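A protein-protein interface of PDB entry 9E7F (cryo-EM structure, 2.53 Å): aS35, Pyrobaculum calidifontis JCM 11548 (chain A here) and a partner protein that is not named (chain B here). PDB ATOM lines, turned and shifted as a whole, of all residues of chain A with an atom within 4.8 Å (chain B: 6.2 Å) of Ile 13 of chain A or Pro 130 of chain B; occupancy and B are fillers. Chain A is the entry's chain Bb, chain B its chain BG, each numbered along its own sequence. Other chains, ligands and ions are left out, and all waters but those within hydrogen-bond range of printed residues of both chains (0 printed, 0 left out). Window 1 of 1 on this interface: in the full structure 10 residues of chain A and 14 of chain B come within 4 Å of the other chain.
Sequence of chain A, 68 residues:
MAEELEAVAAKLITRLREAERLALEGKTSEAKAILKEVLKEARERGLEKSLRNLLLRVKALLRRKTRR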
ATOM      1  N   GLU A   6       4.183  11.541  -7.746  1.00  0.00           N
ATOM      2  CA  GLU A   6       3.078  12.371  -7.280  1.00  0.00           C
ATOM      3  C   GLU A   6       2.864  13.567  -8.193  1.00  0.00           C
ATOM      4  O   GLU A   6       1.732  14.036  -8.351  1.00  0.00           O
ATOM      5  CB  GLU A   6       3.328  12.843  -5.844  1.00  0.00           C
ATOM      6  CG  GLU A   6       3.843  11.760  -4.901  1.00  0.00           C
ATOM      7  CD  GLU A   6       2.802  11.294  -3.899  1.00  0.00           C
ATOM      8  OE1 GLU A   6       1.683  11.845  -3.889  1.00  0.00           O
ATOM      9  OE2 GLU A   6       3.105  10.369  -3.115  1.00  0.00           O
ATOM     10  N   ALA A   9       0.995  12.192 -11.202  1.00  0.00           N
ATOM     11  CA  ALA A   9      -0.353  11.756 -10.855  1.00  0.00           C
ATOM     12  C   ALA A   9      -1.270  12.940 -10.585  1.00  0.00           C
ATOM     13  O   ALA A   9      -2.472  12.870 -10.864  1.00  0.00           O
ATOM     14  CB  ALA A   9      -0.310  10.824  -9.647  1.00  0.00           C
ATOM     15  N   ALA A  10      -0.726  14.025 -10.032  1.00  0.00           N
ATOM     16  CA  ALA A  10      -1.547  15.178  -9.673  1.00  0.00           C
ATOM     17  C   ALA A  10      -2.152  15.833 -10.908  1.00  0.00           C
ATOM     18  O   ALA A  10      -3.338  16.180 -10.928  1.00  0.00           O
ATOM     19  CB  ALA A  10      -0.712  16.185  -8.884  1.00  0.00           C
ATOM     20  N   LYS A  11      -1.345  16.010 -11.951  1.00  0.00           N
ATOM     21  CA  LYS A  11      -1.867  16.514 -13.215  1.00  0.00           C
ATOM     22  C   LYS A  11      -2.777  15.491 -13.876  1.00  0.00           C
ATOM     23  O   LYS A  11      -3.779  15.855 -14.501  1.00  0.00           O
ATOM     24  CB  LYS A  11      -0.706  16.877 -14.135  1.00  0.00           C
ATOM     25  CG  LYS A  11       0.481  15.937 -13.982  1.00  0.00           C
ATOM     26  CD  LYS A  11       1.308  15.857 -15.250  1.00  0.00           C
ATOM     27  CE  LYS A  11       0.480  15.398 -16.432  1.00  0.00           C
ATOM     28  NZ  LYS A  11       1.346  15.089 -17.604  1.00  0.00           N
ATOM     29  N   LEU A  12      -2.427  14.205 -13.763  1.00  0.00           N
ATOM     30  CA  LEU A  12      -3.266  13.147 -14.316  1.00  0.00           C
ATOM     31  C   LEU A  12      -4.631  13.129 -13.651  1.00  0.00           C
ATOM     32  O   LEU A  12      -5.663  13.047 -14.326  1.00  0.00           O
ATOM     33  CB  LEU A  12      -2.588  11.791 -14.142  1.00  0.00           C
ATOM     34  CG  LEU A  12      -1.590  11.339 -15.195  1.00  0.00           C
ATOM     35  CD1 LEU A  12      -1.105   9.960 -14.832  1.00  0.00           C
ATOM     36  CD2 LEU A  12      -2.245  11.340 -16.554  1.00  0.00           C
ATOM     37  N   ILE A  13      -4.655  13.210 -12.320  1.00  0.00           N
ATOM     38  CA  ILE A  13      -5.928  13.295 -11.619  1.00  0.00           C
ATOM     39  C   ILE A  13      -6.623  14.602 -11.959  1.00  0.00           C
ATOM     40  O   ILE A  13      -7.842  14.640 -12.147  1.00  0.00           O
ATOM     41  CB  ILE A  13      -5.732  13.125 -10.103  1.00  0.00           C
ATOM     42  CG1 ILE A  13      -5.240  11.710  -9.799  1.00  0.00           C
ATOM     43  CG2 ILE A  13      -7.035  13.380  -9.382  1.00  0.00           C
ATOM     44  CD1 ILE A  13      -4.473  11.583  -8.510  1.00  0.00           C
ATOM     45  N   THR A  14      -5.852  15.685 -12.080  1.00  0.00           N
ATOM     46  CA  THR A  14      -6.420  16.961 -12.502  1.00  0.00           C
ATOM     47  C   THR A  14      -6.997  16.866 -13.907  1.00  0.00           C
ATOM     48  O   THR A  14      -8.081  17.390 -14.184  1.00  0.00           O
ATOM     49  CB  THR A  14      -5.356  18.051 -12.442  1.00  0.00           C
ATOM     50  OG1 THR A  14      -5.188  18.485 -11.088  1.00  0.00           O
ATOM     51  CG2 THR A  14      -5.763  19.224 -13.308  1.00  0.00           C
ATOM     52  N   ARG A  15      -6.292  16.182 -14.807  1.00  0.00           N
ATOM     53  CA  ARG A  15      -6.805  16.035 -16.161  1.00  0.00           C
ATOM     54  C   ARG A  15      -7.965  15.050 -16.214  1.00  0.00           C
ATOM     55  O   ARG A  15      -8.852  15.176 -17.065  1.00  0.00           O
ATOM     56  CB  ARG A  15      -5.686  15.619 -17.109  1.00  0.00           C
ATOM     57  CG  ARG A  15      -5.932  16.059 -18.535  1.00  0.00           C
ATOM     58  CD  ARG A  15      -4.722  16.116 -19.494  1.00  0.00           C
ATOM     59  NE  ARG A  15      -3.548  16.875 -19.064  1.00  0.00           N
ATOM     60  CZ  ARG A  15      -2.681  16.538 -18.115  1.00  0.00           C
ATOM     61  NH1 ARG A  15      -2.651  15.324 -17.594  1.00  0.00           N
ATOM     62  NH2 ARG A  15      -1.766  17.425 -17.735  1.00  0.00           N
ATOM     63  N   LEU A  16      -7.986  14.067 -15.314  1.00  0.00           N
ATOM     64  CA  LEU A  16      -9.105  13.133 -15.297  1.00  0.00           C
ATOM     65  C   LEU A  16     -10.373  13.798 -14.776  1.00  0.00           C
ATOM     66  O   LEU A  16     -11.456  13.595 -15.332  1.00  0.00           O
ATOM     67  CB  LEU A  16      -8.760  11.900 -14.466  1.00  0.00           C
ATOM     68  CG  LEU A  16      -8.113  10.733 -15.221  1.00  0.00           C
ATOM     69  CD1 LEU A  16      -8.070   9.493 -14.350  1.00  0.00           C
ATOM     70  CD2 LEU A  16      -8.849  10.444 -16.518  1.00  0.00           C
ATOM     71  N   ARG A  17     -10.260  14.599 -13.713  1.00  0.00           N
ATOM     72  CA  ARG A  17     -11.444  15.263 -13.172  1.00  0.00           C
ATOM     73  C   ARG A  17     -11.991  16.317 -14.123  1.00  0.00           C
ATOM     74  O   ARG A  17     -13.210  16.510 -14.198  1.00  0.00           O
ATOM     75  CB  ARG A  17     -11.152  15.884 -11.806  1.00  0.00           C
ATOM     76  CG  ARG A  17     -10.460  14.977 -10.812  1.00  0.00           C
ATOM     77  CD  ARG A  17     -11.337  13.793 -10.470  1.00  0.00           C
ATOM     78  NE  ARG A  17     -10.820  13.033  -9.338  1.00  0.00           N
ATOM     79  CZ  ARG A  17     -11.580  12.354  -8.491  1.00  0.00           C
ATOM     80  NH1 ARG A  17     -12.898  12.350  -8.596  1.00  0.00           N
ATOM     81  NH2 ARG A  17     -11.005  11.661  -7.516  1.00  0.00           N
ATOM     82  N   LEU A  51      -5.456   5.108 -10.703  1.00  0.00           N
ATOM     83  CA  LEU A  51      -6.565   5.941 -11.133  1.00  0.00           C
ATOM     84  C   LEU A  51      -7.805   5.124 -11.461  1.00  0.00           C
ATOM     85  O   LEU A  51      -8.629   5.564 -12.270  1.00  0.00           O
ATOM     86  CB  LEU A  51      -6.153   6.766 -12.351  1.00  0.00           C
ATOM     87  CG  LEU A  51      -4.755   7.385 -12.367  1.00  0.00           C
ATOM     88  CD1 LEU A  51      -4.667   8.400 -13.482  1.00  0.00           C
ATOM     89  CD2 LEU A  51      -4.410   8.041 -11.042  1.00  0.00           C
ATOM     90  N   ASP B  10      -8.456  12.419   0.653  1.00  0.00           N
ATOM     91  CA  ASP B  10      -8.643  13.449  -0.353  1.00  0.00           C
ATOM     92  C   ASP B  10      -9.792  13.062  -1.263  1.00  0.00           C
ATOM     93  O   ASP B  10      -9.694  12.038  -1.958  1.00  0.00           O
ATOM     94  CB  ASP B  10      -7.369  13.635  -1.166  1.00  0.00           C
ATOM     95  CG  ASP B  10      -7.482  14.750  -2.177  1.00  0.00           C
ATOM     96  OD1 ASP B  10      -8.058  14.521  -3.261  1.00  0.00           O
ATOM     97  OD2 ASP B  10      -6.997  15.859  -1.884  1.00  0.00           O
ATOM     98  N   LEU B  12     -10.668  14.511  -4.036  1.00  0.00           N
ATOM     99  CA  LEU B  12     -10.331  14.739  -5.432  1.00  0.00           C
ATOM    100  C   LEU B  12      -9.312  13.755  -5.979  1.00  0.00           C
ATOM    101  O   LEU B  12      -9.121  13.706  -7.198  1.00  0.00           O
ATOM    102  CB  LEU B  12      -9.805  16.163  -5.632  1.00  0.00           C
ATOM    103  CG  LEU B  12     -10.878  17.241  -5.765  1.00  0.00           C
ATOM    104  CD1 LEU B  12     -10.246  18.560  -6.153  1.00  0.00           C
ATOM    105  CD2 LEU B  12     -11.932  16.825  -6.776  1.00  0.00           C
ATOM    106  N   SER B  13      -8.688  12.944  -5.131  1.00  0.00           N
ATOM    107  CA  SER B  13      -7.822  11.880  -5.616  1.00  0.00           C
ATOM    108  C   SER B  13      -8.251  10.497  -5.160  1.00  0.00           C
ATOM    109  O   SER B  13      -7.743   9.509  -5.693  1.00  0.00           O
ATOM    110  CB  SER B  13      -6.374  12.115  -5.172  1.00  0.00           C
ATOM    111  OG  SER B  13      -5.827  10.926  -4.636  1.00  0.00           O
ATOM    112  N   LYS B  15      -7.559   9.059  -2.341  1.00  0.00           N
ATOM    113  CA  LYS B  15      -6.507   8.444  -1.551  1.00  0.00           C
ATOM    114  C   LYS B  15      -6.550   8.995  -0.134  1.00  0.00           C
ATOM    115  O   LYS B  15      -7.120  10.060   0.126  1.00  0.00           O
ATOM    116  CB  LYS B  15      -5.127   8.684  -2.167  1.00  0.00           C
ATOM    117  CG  LYS B  15      -4.721   7.659  -3.206  1.00  0.00           C
ATOM    118  CD  LYS B  15      -5.540   7.779  -4.472  1.00  0.00           C
ATOM    119  CE  LYS B  15      -4.987   6.879  -5.560  1.00  0.00           C
ATOM    120  NZ  LYS B  15      -4.674   5.530  -5.029  1.00  0.00           N
ATOM    121  N   ARG B  17      -4.169   9.614   3.499  1.00  0.00           N
ATOM    122  CA  ARG B  17      -2.884   9.692   4.178  1.00  0.00           C
ATOM    123  C   ARG B  17      -3.122   9.659   5.678  1.00  0.00           C
ATOM    124  O   ARG B  17      -4.022  10.337   6.183  1.00  0.00           O
ATOM    125  CB  ARG B  17      -2.121  10.953   3.776  1.00  0.00           C
ATOM    126  CG  ARG B  17      -0.617  10.760   3.725  1.00  0.00           C
ATOM    127  CD  ARG B  17      -0.244   9.507   2.928  1.00  0.00           C
ATOM    128  NE  ARG B  17      -0.209   9.707   1.481  1.00  0.00           N
ATOM    129  CZ  ARG B  17       0.588  10.555   0.839  1.00  0.00           C
ATOM    130  NH1 ARG B  17       1.484  11.289   1.479  1.00  0.00           N
ATOM    131  NH2 ARG B  17       0.496  10.653  -0.483  1.00  0.00           N
ATOM    132  N   PRO B 127      -4.435  17.347  -6.909  1.00  0.00           N
ATOM    133  CA  PRO B 127      -4.853  16.707  -5.658  1.00  0.00           C
ATOM    134  C   PRO B 127      -3.837  16.897  -4.545  1.00  0.00           C
ATOM    135  O   PRO B 127      -2.629  16.741  -4.736  1.00  0.00           O
ATOM    136  CB  PRO B 127      -4.944  15.223  -6.048  1.00  0.00           C
ATOM    137  CG  PRO B 127      -5.012  15.224  -7.541  1.00  0.00           C
ATOM    138  CD  PRO B 127      -4.120  16.346  -7.935  1.00  0.00           C
ATOM    139  N   ALA B 128      -4.347  17.219  -3.354  1.00  0.00           N
ATOM    140  CA  ALA B 128      -3.481  17.347  -2.189  1.00  0.00           C
ATOM    141  C   ALA B 128      -2.851  16.022  -1.789  1.00  0.00           C
ATOM    142  O   ALA B 128      -1.772  16.020  -1.191  1.00  0.00           O
ATOM    143  CB  ALA B 128      -4.259  17.924  -1.008  1.00  0.00           C
ATOM    144  N   ILE B 129      -3.501  14.905  -2.100  1.00  0.00           N
ATOM    145  CA  ILE B 129      -2.955  13.574  -1.851  1.00  0.00           C
ATOM    146  C   ILE B 129      -3.074  12.770  -3.139  1.00  0.00           C
ATOM    147  O   ILE B 129      -3.996  11.955  -3.278  1.00  0.00           O
ATOM    148  CB  ILE B 129      -3.678  12.878  -0.689  1.00  0.00           C
ATOM    149  CG1 ILE B 129      -3.657  13.764   0.554  1.00  0.00           C
ATOM    150  CG2 ILE B 129      -3.037  11.536  -0.396  1.00  0.00           C
ATOM    151  CD1 ILE B 129      -4.592  13.301   1.639  1.00  0.00           C
ATOM    152  N   PRO B 130      -2.182  12.973  -4.109  1.00  0.00           N
ATOM    153  CA  PRO B 130      -2.365  12.313  -5.408  1.00  0.00           C
ATOM    154  C   PRO B 130      -2.108  10.820  -5.378  1.00  0.00           C
ATOM    155  O   PRO B 130      -2.547  10.114  -6.295  1.00  0.00           O
ATOM    156  CB  PRO B 130      -1.368  13.044  -6.313  1.00  0.00           C
ATOM    157  CG  PRO B 130      -0.317  13.533  -5.391  1.00  0.00           C
ATOM    158  CD  PRO B 130      -0.965  13.798  -4.062  1.00  0.00           C
ATOM    159  N   LEU B 131      -1.413  10.304  -4.370  1.00  0.00           N
ATOM    160  CA  LEU B 131      -1.161   8.874  -4.289  1.00  0.00           C
ATOM    161  C   LEU B 131      -1.103   8.444  -2.834  1.00  0.00           C
ATOM    162  O   LEU B 131      -0.899   9.257  -1.931  1.00  0.00           O
ATOM    163  CB  LEU B 131       0.142   8.474  -4.996  1.00  0.00           C
ATOM    164  CG  LEU B 131       0.204   8.658  -6.510  1.00  0.00           C
ATOM    165  CD1 LEU B 131       1.590   9.104  -6.933  1.00  0.00           C
ATOM    166  CD2 LEU B 131      -0.188   7.373  -7.216  1.00  0.00           C
ATOM    167  N   GLY B 132      -1.301   7.146  -2.622  1.00  0.00           N
ATOM    168  CA  GLY B 132      -1.099   6.573  -1.313  1.00  0.00           C
ATOM    169  C   GLY B 132       0.356   6.253  -1.068  1.00  0.00           C
ATOM    170  O   GLY B 132       1.125   5.976  -1.986  1.00  0.00           O
ATOM    171  N   GLU B 135       0.789   2.558  -1.697  1.00  0.00           N
ATOM    172  CA  GLU B 135       0.641   2.365  -3.135  1.00  0.00           C
ATOM    173  C   GLU B 135       1.876   2.848  -3.882  1.00  0.00           C
ATOM    174  O   GLU B 135       2.378   2.168  -4.783  1.00  0.00           O
ATOM    175  CB  GLU B 135      -0.604   3.098  -3.631  1.00  0.00           C
ATOM    176  CG  GLU B 135      -1.012   2.733  -5.040  1.00  0.00           C
ATOM    177  CD  GLU B 135      -2.270   3.447  -5.479  1.00  0.00           C
ATOM    178  OE1 GLU B 135      -2.382   4.663  -5.218  1.00  0.00           O
ATOM    179  OE2 GLU B 135      -3.142   2.799  -6.092  1.00  0.00           O
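O of Leu 12 of chain B lies within hydrogen-bond range of NH2 of Arg 17 of chain A, at 2.8 Å.
The side-chain carboxylate (OE2) of Glu 6 of chain A is in salt-bridge range of the guanidinium group (NH2) of Arg 17 of chain B (3.7 Å).
The backbone NH of Leu 131 of chain B lies within hydrogen-bond range of the side-chain carboxylate of Glu 6 of chain A, at 3.5 Å.
The side-chain carboxylate (OD1) of Asp 10 of chain B lies within hydrogen-bond range of the backbone NH (N) of Leu 12 of chain B, 2.7 Å away.
The side-chain carboxylate (OD1) of Asp 10 of chain B sits at hydrogen-bond distance from the backbone NH (N) of Ser 13 of chain B (2.5 Å).
The side-chain hydroxyl (OG) of Ser 13 of chain B sits close to the backbone NH (N) of Lys 15 of chain B (3.4 Å).
The side-chain hydroxyl (OG) of Ser 13 of chain B sits at hydrogen-bond distance from the backbone carbonyl oxygen (O) of Ile 129 of chain B (2.5 Å).
The guanidinium group (NH2) of Arg 17 of chain B sits at hydrogen-bond distance from the backbone carbonyl oxygen (O) of Leu 131 of chain B, at 2.4 Å.
O of Ala 10 of chain A lies within hydrogen-bond range of OG1 of Thr 14 of chain A.
Glu 6 of chain A touches Pro 130 of chain B (OE1 to CG, 3.0 Å).
CD1 of Leu 131 of chain B touches CB of Ala 9 of chain A, at 3.7 Å.
O of Ala 10 of chain A touches CD of Pro 127 of chain B (3.1 Å).
N of Ala 10 of chain A touches CB of Pro 130 of chain B, at 3.9 Å.
Leu 12 of chain B touches Ile 13 of chain A (O to CG2, 3.0 Å).
CB of Ser 13 of chain B touches CD1 of Ile 13 of chain A (3.9 Å).
CG of Pro 127 of chain B touches CG2 of Ile 13 of chain A (3.3 Å).
Ile 13 of chain A touches Pro 130 of chain B.
Thr 14 of chain A touches Pro 127 of chain B (OG1 to CD, 3.96 Å).
Arg 17 of chain A touches Ser 13 of chain B.
Of the printed residues of chain B, Glu 6 of chain A touches Arg 17 (3.7 Å), Pro 130 (3.0 Å) and Leu 131 (3.5 Å).
Of the printed residues of chain B, Ala 10 of chain A touches Pro 127 (3.1 Å) and Pro 130 (3.9 Å).
Printed residues of chain A within 4 Å of Leu 12 of chain B: Ile 13 and Arg 17.
Of the printed residues of chain A, Ser 13 of chain B touches Ile 13 (3.9 Å) and Arg 17 (3.6 Å).
Ile 129 of chain B touches none of the printed residues of chain A.
Pro 130 of chain B touches just these residues of chain A: Glu 6, Ala 10 and Ile 13.
Gly 132 of chain B touches none of the printed residues of chain A.
The nearest residue of chain A that does not touch Pro 130 of chain B is Ala 9 of chain A (4.1 Å).
The nearest printed residue of chain B that does not touch Ala 10 of chain A is Leu 131 of chain B (6.3 Å).
Printed residues of chain B that touch a printed residue of chain A: Leu 12, Ser 13, Arg 17, Pro 127, Pro 130 and Leu 131.
Hydrophobic or aromatic side chains of chain B that line the printed part of chain A: Pro 127, Pro 130 and Leu 131.
Of the 11 printed residues of chain A, 6 touch a printed residue of chain B.
Hydrophobic or aromatic side chains of chain A within 4 Å of the printed part of chain B: Ala 9, Ala 10 and Ile 13.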
